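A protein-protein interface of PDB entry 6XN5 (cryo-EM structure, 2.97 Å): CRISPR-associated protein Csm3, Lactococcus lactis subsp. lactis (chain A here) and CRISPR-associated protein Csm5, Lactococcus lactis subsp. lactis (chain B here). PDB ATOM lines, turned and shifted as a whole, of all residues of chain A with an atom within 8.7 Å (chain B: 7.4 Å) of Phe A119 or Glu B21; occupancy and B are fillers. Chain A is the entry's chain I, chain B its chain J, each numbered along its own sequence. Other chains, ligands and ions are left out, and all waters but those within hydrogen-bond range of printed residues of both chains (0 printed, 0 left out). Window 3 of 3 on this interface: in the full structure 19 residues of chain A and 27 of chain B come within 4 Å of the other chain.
The backbone carbonyl oxygen of Ile A135 sits at hydrogen-bond distance from the backbone NH of Lys A118 (3.3 Å).
NZ of Lys A118 touches CB of Pro B127, 3.8 Å away.
O of Gly B19 touches CB of Phe A119, at 3.3 Å.
Gly B20 touches Phe A119.
Phe A119 touches Glu B21 (CZ to OE2, 3.2 Å).
Gly B18 touches Asn A121 (CA to OD1, 3.5 Å).
OD1 of Asn A121 touches N of Gly B19, 3.7 Å away.
Of the printed residues of chain B, Lys A118 touches Pro B127.
Phe A119 touches three residues of chain B.
Of the printed residues of chain A, Gly B19 touches Phe A119 (3.3 Å) and Asn A121 (3.7 Å).
Of chain A, only Phe A119 (3.2 Å) comes within 4 Å of Glu B21.
Of the printed residues of chain A, Pro B127 touches Lys A118.
The nearest residue of chain A that does not touch Glu B21 is Gln A134 (6.5 Å).
Hydrophobic or aromatic side chains of chain A within 4 Å of the printed part of chain B: Phe A119.
Printed residues of chain B that touch a printed residue of chain A: Gly B18, Gly B19, Gly B20, Glu B21 and Pro B127.
Hydrophobic or aromatic side chains of chain B within 4 Å of the printed part of chain A: Pro B127.
Among the printed residues, 6 pairs touch across the chains.
Among the printed residues, no Asp or Glu carboxylate lies within 4 Å of a Lys or Arg side-chain nitrogen of the other chain.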
ATOM      1  N   ALA A  28       0.612 -12.926 -16.429  1.00  0.00           N
ATOM      2  CA  ALA A  28       0.544 -11.537 -16.882  1.00  0.00           C
ATOM      3  C   ALA A  28       1.118 -11.380 -18.288  1.00  0.00           C
ATOM      4  O   ALA A  28       1.940 -10.505 -18.556  1.00  0.00           O
ATOM      5  CB  ALA A  28       1.266 -10.634 -15.890  1.00  0.00           C
ATOM      6  N   GLU A 116      10.808 -11.283 -25.334  1.00  0.00           N
ATOM      7  CA  GLU A 116      10.647  -9.900 -24.914  1.00  0.00           C
ATOM      8  C   GLU A 116       9.181  -9.616 -24.632  1.00  0.00           C
ATOM      9  O   GLU A 116       8.305  -9.996 -25.413  1.00  0.00           O
ATOM     10  CB  GLU A 116      11.162  -8.936 -25.988  1.00  0.00           C
ATOM     11  CG  GLU A 116      11.106  -7.471 -25.603  1.00  0.00           C
ATOM     12  CD  GLU A 116      11.673  -6.567 -26.679  1.00  0.00           C
ATOM     13  OE1 GLU A 116      12.088  -7.089 -27.734  1.00  0.00           O
ATOM     14  OE2 GLU A 116      11.710  -5.337 -26.468  1.00  0.00           O
ATOM     15  N   VAL A 117       8.919  -8.947 -23.515  1.00  0.00           N
ATOM     16  CA  VAL A 117       7.585  -8.479 -23.167  1.00  0.00           C
ATOM     17  C   VAL A 117       7.611  -6.954 -23.159  1.00  0.00           C
ATOM     18  O   VAL A 117       8.615  -6.344 -22.767  1.00  0.00           O
ATOM     19  CB  VAL A 117       7.099  -9.076 -21.827  1.00  0.00           C
ATOM     20  CG1 VAL A 117       7.941  -8.619 -20.630  1.00  0.00           C
ATOM     21  CG2 VAL A 117       5.620  -8.780 -21.599  1.00  0.00           C
ATOM     22  N   LYS A 118       6.560  -6.343 -23.690  1.00  0.00           N
ATOM     23  CA  LYS A 118       6.432  -4.897 -23.681  1.00  0.00           C
ATOM     24  C   LYS A 118       5.049  -4.508 -23.181  1.00  0.00           C
ATOM     25  O   LYS A 118       4.071  -5.239 -23.366  1.00  0.00           O
ATOM     26  CB  LYS A 118       6.692  -4.296 -25.070  1.00  0.00           C
ATOM     27  CG  LYS A 118       5.813  -4.836 -26.176  1.00  0.00           C
ATOM     28  CD  LYS A 118       6.070  -4.112 -27.487  1.00  0.00           C
ATOM     29  CE  LYS A 118       5.260  -2.834 -27.579  1.00  0.00           C
ATOM     30  NZ  LYS A 118       5.253  -2.268 -28.952  1.00  0.00           N
ATOM     31  N   PHE A 119       4.984  -3.353 -22.528  1.00  0.00           N
ATOM     32  CA  PHE A 119       3.745  -2.846 -21.945  1.00  0.00           C
ATOM     33  C   PHE A 119       3.084  -1.941 -22.973  1.00  0.00           C
ATOM     34  O   PHE A 119       3.347  -0.741 -23.039  1.00  0.00           O
ATOM     35  CB  PHE A 119       4.025  -2.108 -20.643  1.00  0.00           C
ATOM     36  CG  PHE A 119       4.426  -3.005 -19.499  1.00  0.00           C
ATOM     37  CD1 PHE A 119       5.724  -3.481 -19.386  1.00  0.00           C
ATOM     38  CD2 PHE A 119       3.503  -3.351 -18.522  1.00  0.00           C
ATOM     39  CE1 PHE A 119       6.086  -4.299 -18.336  1.00  0.00           C
ATOM     40  CE2 PHE A 119       3.860  -4.167 -17.467  1.00  0.00           C
ATOM     41  CZ  PHE A 119       5.152  -4.641 -17.376  1.00  0.00           C
ATOM     42  N   GLU A 120       2.217  -2.522 -23.792  1.00  0.00           N
ATOM     43  CA  GLU A 120       1.587  -1.782 -24.882  1.00  0.00           C
ATOM     44  C   GLU A 120       0.318  -1.117 -24.359  1.00  0.00           C
ATOM     45  O   GLU A 120      -0.743  -1.735 -24.274  1.00  0.00           O
ATOM     46  CB  GLU A 120       1.291  -2.708 -26.054  1.00  0.00           C
ATOM     47  CG  GLU A 120       1.087  -1.985 -27.366  1.00  0.00           C
ATOM     48  CD  GLU A 120      -0.358  -1.645 -27.615  1.00  0.00           C
ATOM     49  OE1 GLU A 120      -1.232  -2.413 -27.166  1.00  0.00           O
ATOM     50  OE2 GLU A 120      -0.622  -0.609 -28.259  1.00  0.00           O
ATOM     51  N   ASN A 121       0.430   0.167 -24.018  1.00  0.00           N
ATOM     52  CA  ASN A 121      -0.712   0.931 -23.535  1.00  0.00           C
ATOM     53  C   ASN A 121      -1.669   1.239 -24.686  1.00  0.00           C
ATOM     54  O   ASN A 121      -1.343   1.084 -25.862  1.00  0.00           O
ATOM     55  CB  ASN A 121      -0.253   2.234 -22.882  1.00  0.00           C
ATOM     56  CG  ASN A 121       0.985   2.060 -22.028  1.00  0.00           C
ATOM     57  OD1 ASN A 121       1.982   2.756 -22.214  1.00  0.00           O
ATOM     58  ND2 ASN A 121       0.928   1.129 -21.086  1.00  0.00           N
ATOM     59  N   THR A 122      -2.872   1.685 -24.332  1.00  0.00           N
ATOM     60  CA  THR A 122      -3.867   2.042 -25.339  1.00  0.00           C
ATOM     61  C   THR A 122      -4.719   3.180 -24.806  1.00  0.00           C
ATOM     62  O   THR A 122      -5.434   3.003 -23.815  1.00  0.00           O
ATOM     63  CB  THR A 122      -4.742   0.846 -25.697  1.00  0.00           C
ATOM     64  OG1 THR A 122      -3.941  -0.174 -26.300  1.00  0.00           O
ATOM     65  CG2 THR A 122      -5.833   1.263 -26.668  1.00  0.00           C
ATOM     66  N   ASN A 131      -5.258   1.968 -21.140  1.00  0.00           N
ATOM     67  CA  ASN A 131      -5.724   0.586 -21.037  1.00  0.00           C
ATOM     68  C   ASN A 131      -4.521  -0.327 -21.225  1.00  0.00           C
ATOM     69  O   ASN A 131      -4.245  -0.788 -22.339  1.00  0.00           O
ATOM     70  CB  ASN A 131      -6.813   0.289 -22.069  1.00  0.00           C
ATOM     71  CG  ASN A 131      -7.990   1.238 -21.967  1.00  0.00           C
ATOM     72  OD1 ASN A 131      -8.252   2.020 -22.878  1.00  0.00           O
ATOM     73  ND2 ASN A 131      -8.709   1.173 -20.854  1.00  0.00           N
ATOM     74  N   PRO A 132      -3.766  -0.584 -20.154  1.00  0.00           N
ATOM     75  CA  PRO A 132      -2.510  -1.329 -20.293  1.00  0.00           C
ATOM     76  C   PRO A 132      -2.728  -2.796 -20.631  1.00  0.00           C
ATOM     77  O   PRO A 132      -3.725  -3.411 -20.249  1.00  0.00           O
ATOM     78  CB  PRO A 132      -1.849  -1.165 -18.919  1.00  0.00           C
ATOM     79  CG  PRO A 132      -2.502   0.039 -18.331  1.00  0.00           C
ATOM     80  CD  PRO A 132      -3.919  -0.050 -18.794  1.00  0.00           C
ATOM     81  N   ARG A 133      -1.758  -3.350 -21.357  1.00  0.00           N
ATOM     82  CA  ARG A 133      -1.815  -4.715 -21.860  1.00  0.00           C
ATOM     83  C   ARG A 133      -0.393  -5.160 -22.156  1.00  0.00           C
ATOM     84  O   ARG A 133       0.466  -4.327 -22.459  1.00  0.00           O
ATOM     85  CB  ARG A 133      -2.689  -4.789 -23.114  1.00  0.00           C
ATOM     86  CG  ARG A 133      -3.249  -6.160 -23.443  1.00  0.00           C
ATOM     87  CD  ARG A 133      -2.420  -6.836 -24.517  1.00  0.00           C
ATOM     88  NE  ARG A 133      -1.996  -5.886 -25.545  1.00  0.00           N
ATOM     89  CZ  ARG A 133      -2.758  -5.453 -26.546  1.00  0.00           C
ATOM     90  NH1 ARG A 133      -4.003  -5.883 -26.690  1.00  0.00           N
ATOM     91  NH2 ARG A 133      -2.261  -4.586 -27.415  1.00  0.00           N
ATOM     92  N   GLN A 134      -0.141  -6.458 -22.056  1.00  0.00           N
ATOM     93  CA  GLN A 134       1.192  -7.003 -22.258  1.00  0.00           C
ATOM     94  C   GLN A 134       1.175  -8.025 -23.386  1.00  0.00           C
ATOM     95  O   GLN A 134       0.375  -8.965 -23.366  1.00  0.00           O
ATOM     96  CB  GLN A 134       1.709  -7.644 -20.970  1.00  0.00           C
ATOM     97  CG  GLN A 134       1.865  -6.670 -19.814  1.00  0.00           C
ATOM     98  CD  GLN A 134       1.677  -7.335 -18.463  1.00  0.00           C
ATOM     99  OE1 GLN A 134       2.638  -7.548 -17.724  1.00  0.00           O
ATOM    100  NE2 GLN A 134       0.435  -7.674 -18.137  1.00  0.00           N
ATOM    101  N   ILE A 135       2.061  -7.842 -24.364  1.00  0.00           N
ATOM    102  CA  ILE A 135       2.265  -8.796 -25.445  1.00  0.00           C
ATOM    103  C   ILE A 135       3.679  -9.342 -25.333  1.00  0.00           C
ATOM    104  O   ILE A 135       4.562  -8.684 -24.771  1.00  0.00           O
ATOM    105  CB  ILE A 135       2.030  -8.169 -26.835  1.00  0.00           C
ATOM    106  CG1 ILE A 135       2.999  -7.015 -27.081  1.00  0.00           C
ATOM    107  CG2 ILE A 135       0.598  -7.696 -26.971  1.00  0.00           C
ATOM    108  CD1 ILE A 135       2.994  -6.496 -28.496  1.00  0.00           C
ATOM    109  N   GLU A 136       3.886 -10.553 -25.832  1.00  0.00           N
ATOM    110  CA  GLU A 136       5.176 -11.217 -25.758  1.00  0.00           C
ATOM    111  C   GLU A 136       5.746 -11.380 -27.161  1.00  0.00           C
ATOM    112  O   GLU A 136       5.160 -12.073 -27.998  1.00  0.00           O
ATOM    113  CB  GLU A 136       5.040 -12.578 -25.074  1.00  0.00           C
ATOM    114  CG  GLU A 136       6.347 -13.310 -24.876  1.00  0.00           C
ATOM    115  CD  GLU A 136       6.170 -14.628 -24.156  1.00  0.00           C
ATOM    116  OE1 GLU A 136       5.018 -14.975 -23.832  1.00  0.00           O
ATOM    117  OE2 GLU A 136       7.180 -15.319 -23.910  1.00  0.00           O
ATOM    118  N   ARG A 137       6.886 -10.748 -27.408  1.00  0.00           N
ATOM    119  CA  ARG A 137       7.605 -10.840 -28.670  1.00  0.00           C
ATOM    120  C   ARG A 137       8.927 -11.561 -28.427  1.00  0.00           C
ATOM    121  O   ARG A 137       9.204 -12.034 -27.323  1.00  0.00           O
ATOM    122  CB  ARG A 137       7.831  -9.447 -29.259  1.00  0.00           C
ATOM    123  CG  ARG A 137       6.571  -8.645 -29.471  1.00  0.00           C
ATOM    124  CD  ARG A 137       6.893  -7.310 -30.105  1.00  0.00           C
ATOM    125  NE  ARG A 137       8.083  -6.706 -29.515  1.00  0.00           N
ATOM    126  CZ  ARG A 137       8.606  -5.551 -29.907  1.00  0.00           C
ATOM    127  NH1 ARG A 137       8.041  -4.864 -30.888  1.00  0.00           N
ATOM    128  NH2 ARG A 137       9.690  -5.077 -29.313  1.00  0.00           N
ATOM    129  N   PHE B  16       7.808  11.176 -23.374  1.00  0.00           N
ATOM    130  CA  PHE B  16       7.763  10.016 -22.483  1.00  0.00           C
ATOM    131  C   PHE B  16       6.606   9.132 -22.940  1.00  0.00           C
ATOM    132  O   PHE B  16       5.482   9.277 -22.454  1.00  0.00           O
ATOM    133  CB  PHE B  16       7.585  10.480 -21.042  1.00  0.00           C
ATOM    134  CG  PHE B  16       7.562   9.377 -20.021  1.00  0.00           C
ATOM    135  CD1 PHE B  16       8.732   8.743 -19.638  1.00  0.00           C
ATOM    136  CD2 PHE B  16       6.373   9.010 -19.405  1.00  0.00           C
ATOM    137  CE1 PHE B  16       8.712   7.740 -18.680  1.00  0.00           C
ATOM    138  CE2 PHE B  16       6.345   8.010 -18.452  1.00  0.00           C
ATOM    139  CZ  PHE B  16       7.516   7.374 -18.088  1.00  0.00           C
ATOM    140  N   ILE B  17       6.884   8.208 -23.858  1.00  0.00           N
ATOM    141  CA  ILE B  17       5.837   7.361 -24.419  1.00  0.00           C
ATOM    142  C   ILE B  17       5.596   6.170 -23.503  1.00  0.00           C
ATOM    143  O   ILE B  17       6.169   5.093 -23.708  1.00  0.00           O
ATOM    144  CB  ILE B  17       6.184   6.888 -25.842  1.00  0.00           C
ATOM    145  CG1 ILE B  17       6.647   8.062 -26.695  1.00  0.00           C
ATOM    146  CG2 ILE B  17       4.974   6.234 -26.492  1.00  0.00           C
ATOM    147  CD1 ILE B  17       5.601   9.119 -26.888  1.00  0.00           C
ATOM    148  N   GLY B  18       4.750   6.369 -22.491  1.00  0.00           N
ATOM    149  CA  GLY B  18       4.257   5.312 -21.627  1.00  0.00           C
ATOM    150  C   GLY B  18       5.328   4.535 -20.897  1.00  0.00           C
ATOM    151  O   GLY B  18       6.035   5.071 -20.041  1.00  0.00           O
ATOM    152  N   GLY B  19       5.473   3.263 -21.266  1.00  0.00           N
ATOM    153  CA  GLY B  19       6.472   2.383 -20.709  1.00  0.00           C
ATOM    154  C   GLY B  19       5.898   1.267 -19.863  1.00  0.00           C
ATOM    155  O   GLY B  19       6.368   0.128 -19.958  1.00  0.00           O
ATOM    156  N   GLY B  20       4.902   1.564 -19.038  1.00  0.00           N
ATOM    157  CA  GLY B  20       4.333   0.541 -18.157  1.00  0.00           C
ATOM    158  C   GLY B  20       5.143   0.242 -16.922  1.00  0.00           C
ATOM    159  O   GLY B  20       4.616   0.296 -15.807  1.00  0.00           O
ATOM    160  N   GLU B  21       6.421  -0.091 -17.089  1.00  0.00           N
ATOM    161  CA  GLU B  21       7.371  -0.068 -15.982  1.00  0.00           C
ATOM    162  C   GLU B  21       7.606   1.394 -15.627  1.00  0.00           C
ATOM    163  O   GLU B  21       8.491   2.068 -16.159  1.00  0.00           O
ATOM    164  CB  GLU B  21       8.677  -0.769 -16.345  1.00  0.00           C
ATOM    165  CG  GLU B  21       8.578  -2.269 -16.564  1.00  0.00           C
ATOM    166  CD  GLU B  21       8.258  -3.022 -15.287  1.00  0.00           C
ATOM    167  OE1 GLU B  21       8.682  -2.567 -14.206  1.00  0.00           O
ATOM    168  OE2 GLU B  21       7.602  -4.079 -15.365  1.00  0.00           O
ATOM    169  N   LYS B  22       6.776   1.900 -14.722  1.00  0.00           N
ATOM    170  CA  LYS B  22       6.929   3.246 -14.194  1.00  0.00           C
ATOM    171  C   LYS B  22       6.529   3.227 -12.728  1.00  0.00           C
ATOM    172  O   LYS B  22       5.500   2.648 -12.369  1.00  0.00           O
ATOM    173  CB  LYS B  22       6.097   4.260 -14.996  1.00  0.00           C
ATOM    174  CG  LYS B  22       4.675   3.833 -15.326  1.00  0.00           C
ATOM    175  CD  LYS B  22       3.976   4.891 -16.166  1.00  0.00           C
ATOM    176  CE  LYS B  22       2.507   4.568 -16.364  1.00  0.00           C
ATOM    177  NZ  LYS B  22       2.312   3.346 -17.191  1.00  0.00           N
ATOM    178  N   LEU B  23       7.353   3.840 -11.886  1.00  0.00           N
ATOM    179  CA  LEU B  23       7.146   3.781 -10.444  1.00  0.00           C
ATOM    180  C   LEU B  23       6.353   4.982  -9.939  1.00  0.00           C
ATOM    181  O   LEU B  23       5.544   4.857  -9.020  1.00  0.00           O
ATOM    182  CB  LEU B  23       8.490   3.691  -9.717  1.00  0.00           C
ATOM    183  CG  LEU B  23       9.318   2.428  -9.964  1.00  0.00           C
ATOM    184  CD1 LEU B  23      10.450   2.697 -10.940  1.00  0.00           C
ATOM    185  CD2 LEU B  23       9.858   1.881  -8.657  1.00  0.00           C
ATOM    186  N   ASN B 114      11.732   7.309 -11.847  1.00  0.00           N
ATOM    187  CA  ASN B 114      10.904   6.755 -12.903  1.00  0.00           C
ATOM    188  C   ASN B 114      11.740   5.858 -13.810  1.00  0.00           C
ATOM    189  O   ASN B 114      12.972   5.854 -13.748  1.00  0.00           O
ATOM    190  CB  ASN B 114      10.255   7.878 -13.724  1.00  0.00           C
ATOM    191  CG  ASN B 114       8.902   7.487 -14.281  1.00  0.00           C
ATOM    192  OD1 ASN B 114       8.444   6.364 -14.092  1.00  0.00           O
ATOM    193  ND2 ASN B 114       8.257   8.415 -14.974  1.00  0.00           N
ATOM    194  N   THR B 115      11.048   5.066 -14.633  1.00  0.00           N
ATOM    195  CA  THR B 115      11.675   4.257 -15.673  1.00  0.00           C
ATOM    196  C   THR B 115      10.891   4.410 -16.975  1.00  0.00           C
ATOM    197  O   THR B 115       9.762   4.904 -16.991  1.00  0.00           O
ATOM    198  CB  THR B 115      11.784   2.767 -15.289  1.00  0.00           C
ATOM    199  OG1 THR B 115      10.484   2.230 -15.043  1.00  0.00           O
ATOM    200  CG2 THR B 115      12.677   2.542 -14.064  1.00  0.00           C
ATOM    201  N   PHE B 116      11.513   3.974 -18.072  1.00  0.00           N
ATOM    202  CA  PHE B 116      11.027   4.200 -19.428  1.00  0.00           C
ATOM    203  C   PHE B 116      11.043   2.887 -20.207  1.00  0.00           C
ATOM    204  O   PHE B 116      11.667   1.907 -19.792  1.00  0.00           O
ATOM    205  CB  PHE B 116      11.887   5.274 -20.135  1.00  0.00           C
ATOM    206  CG  PHE B 116      11.309   5.783 -21.427  1.00  0.00           C
ATOM    207  CD1 PHE B 116       9.960   6.077 -21.534  1.00  0.00           C
ATOM    208  CD2 PHE B 116      12.120   5.956 -22.539  1.00  0.00           C
ATOM    209  CE1 PHE B 116       9.430   6.534 -22.724  1.00  0.00           C
ATOM    210  CE2 PHE B 116      11.595   6.418 -23.736  1.00  0.00           C
ATOM    211  CZ  PHE B 116      10.249   6.708 -23.828  1.00  0.00           C
ATOM    212  N   VAL B 117      10.321   2.868 -21.335  1.00  0.00           N
ATOM    213  CA  VAL B 117      10.373   1.736 -22.252  1.00  0.00           C
ATOM    214  C   VAL B 117      11.748   1.657 -22.908  1.00  0.00           C
ATOM    215  O   VAL B 117      12.315   2.662 -23.357  1.00  0.00           O
ATOM    216  CB  VAL B 117       9.221   1.821 -23.274  1.00  0.00           C
ATOM    217  CG1 VAL B 117       9.257   3.107 -24.108  1.00  0.00           C
ATOM    218  CG2 VAL B 117       9.221   0.599 -24.189  1.00  0.00           C
ATOM    219  N   PRO B 127       8.541   2.830 -29.796  1.00  0.00           N
ATOM    220  CA  PRO B 127       7.799   1.799 -30.529  1.00  0.00           C
ATOM    221  C   PRO B 127       6.873   2.404 -31.570  1.00  0.00           C
ATOM    222  O   PRO B 127       6.432   3.550 -31.467  1.00  0.00           O
ATOM    223  CB  PRO B 127       7.005   1.079 -29.433  1.00  0.00           C
ATOM    224  CG  PRO B 127       7.667   1.474 -28.145  1.00  0.00           C
ATOM    225  CD  PRO B 127       8.192   2.851 -28.369  1.00  0.00           C
ATOM    226  N   GLU B 189      11.546  10.602 -16.025  1.00  0.00           N
ATOM    227  CA  GLU B 189      12.820  10.586 -16.742  1.00  0.00           C
ATOM    228  C   GLU B 189      12.499  10.272 -18.204  1.00  0.00           C
ATOM    229  O   GLU B 189      11.928   9.239 -18.566  1.00  0.00           O
ATOM    230  CB  GLU B 189      13.824   9.629 -16.096  1.00  0.00           C
ATOM    231  CG  GLU B 189      13.476   8.152 -16.026  1.00  0.00           C
ATOM    232  CD  GLU B 189      14.047   7.383 -17.200  1.00  0.00           C
ATOM    233  OE1 GLU B 189      14.991   7.890 -17.836  1.00  0.00           O
ATOM    234  OE2 GLU B 189      13.562   6.273 -17.487  1.00  0.00           O
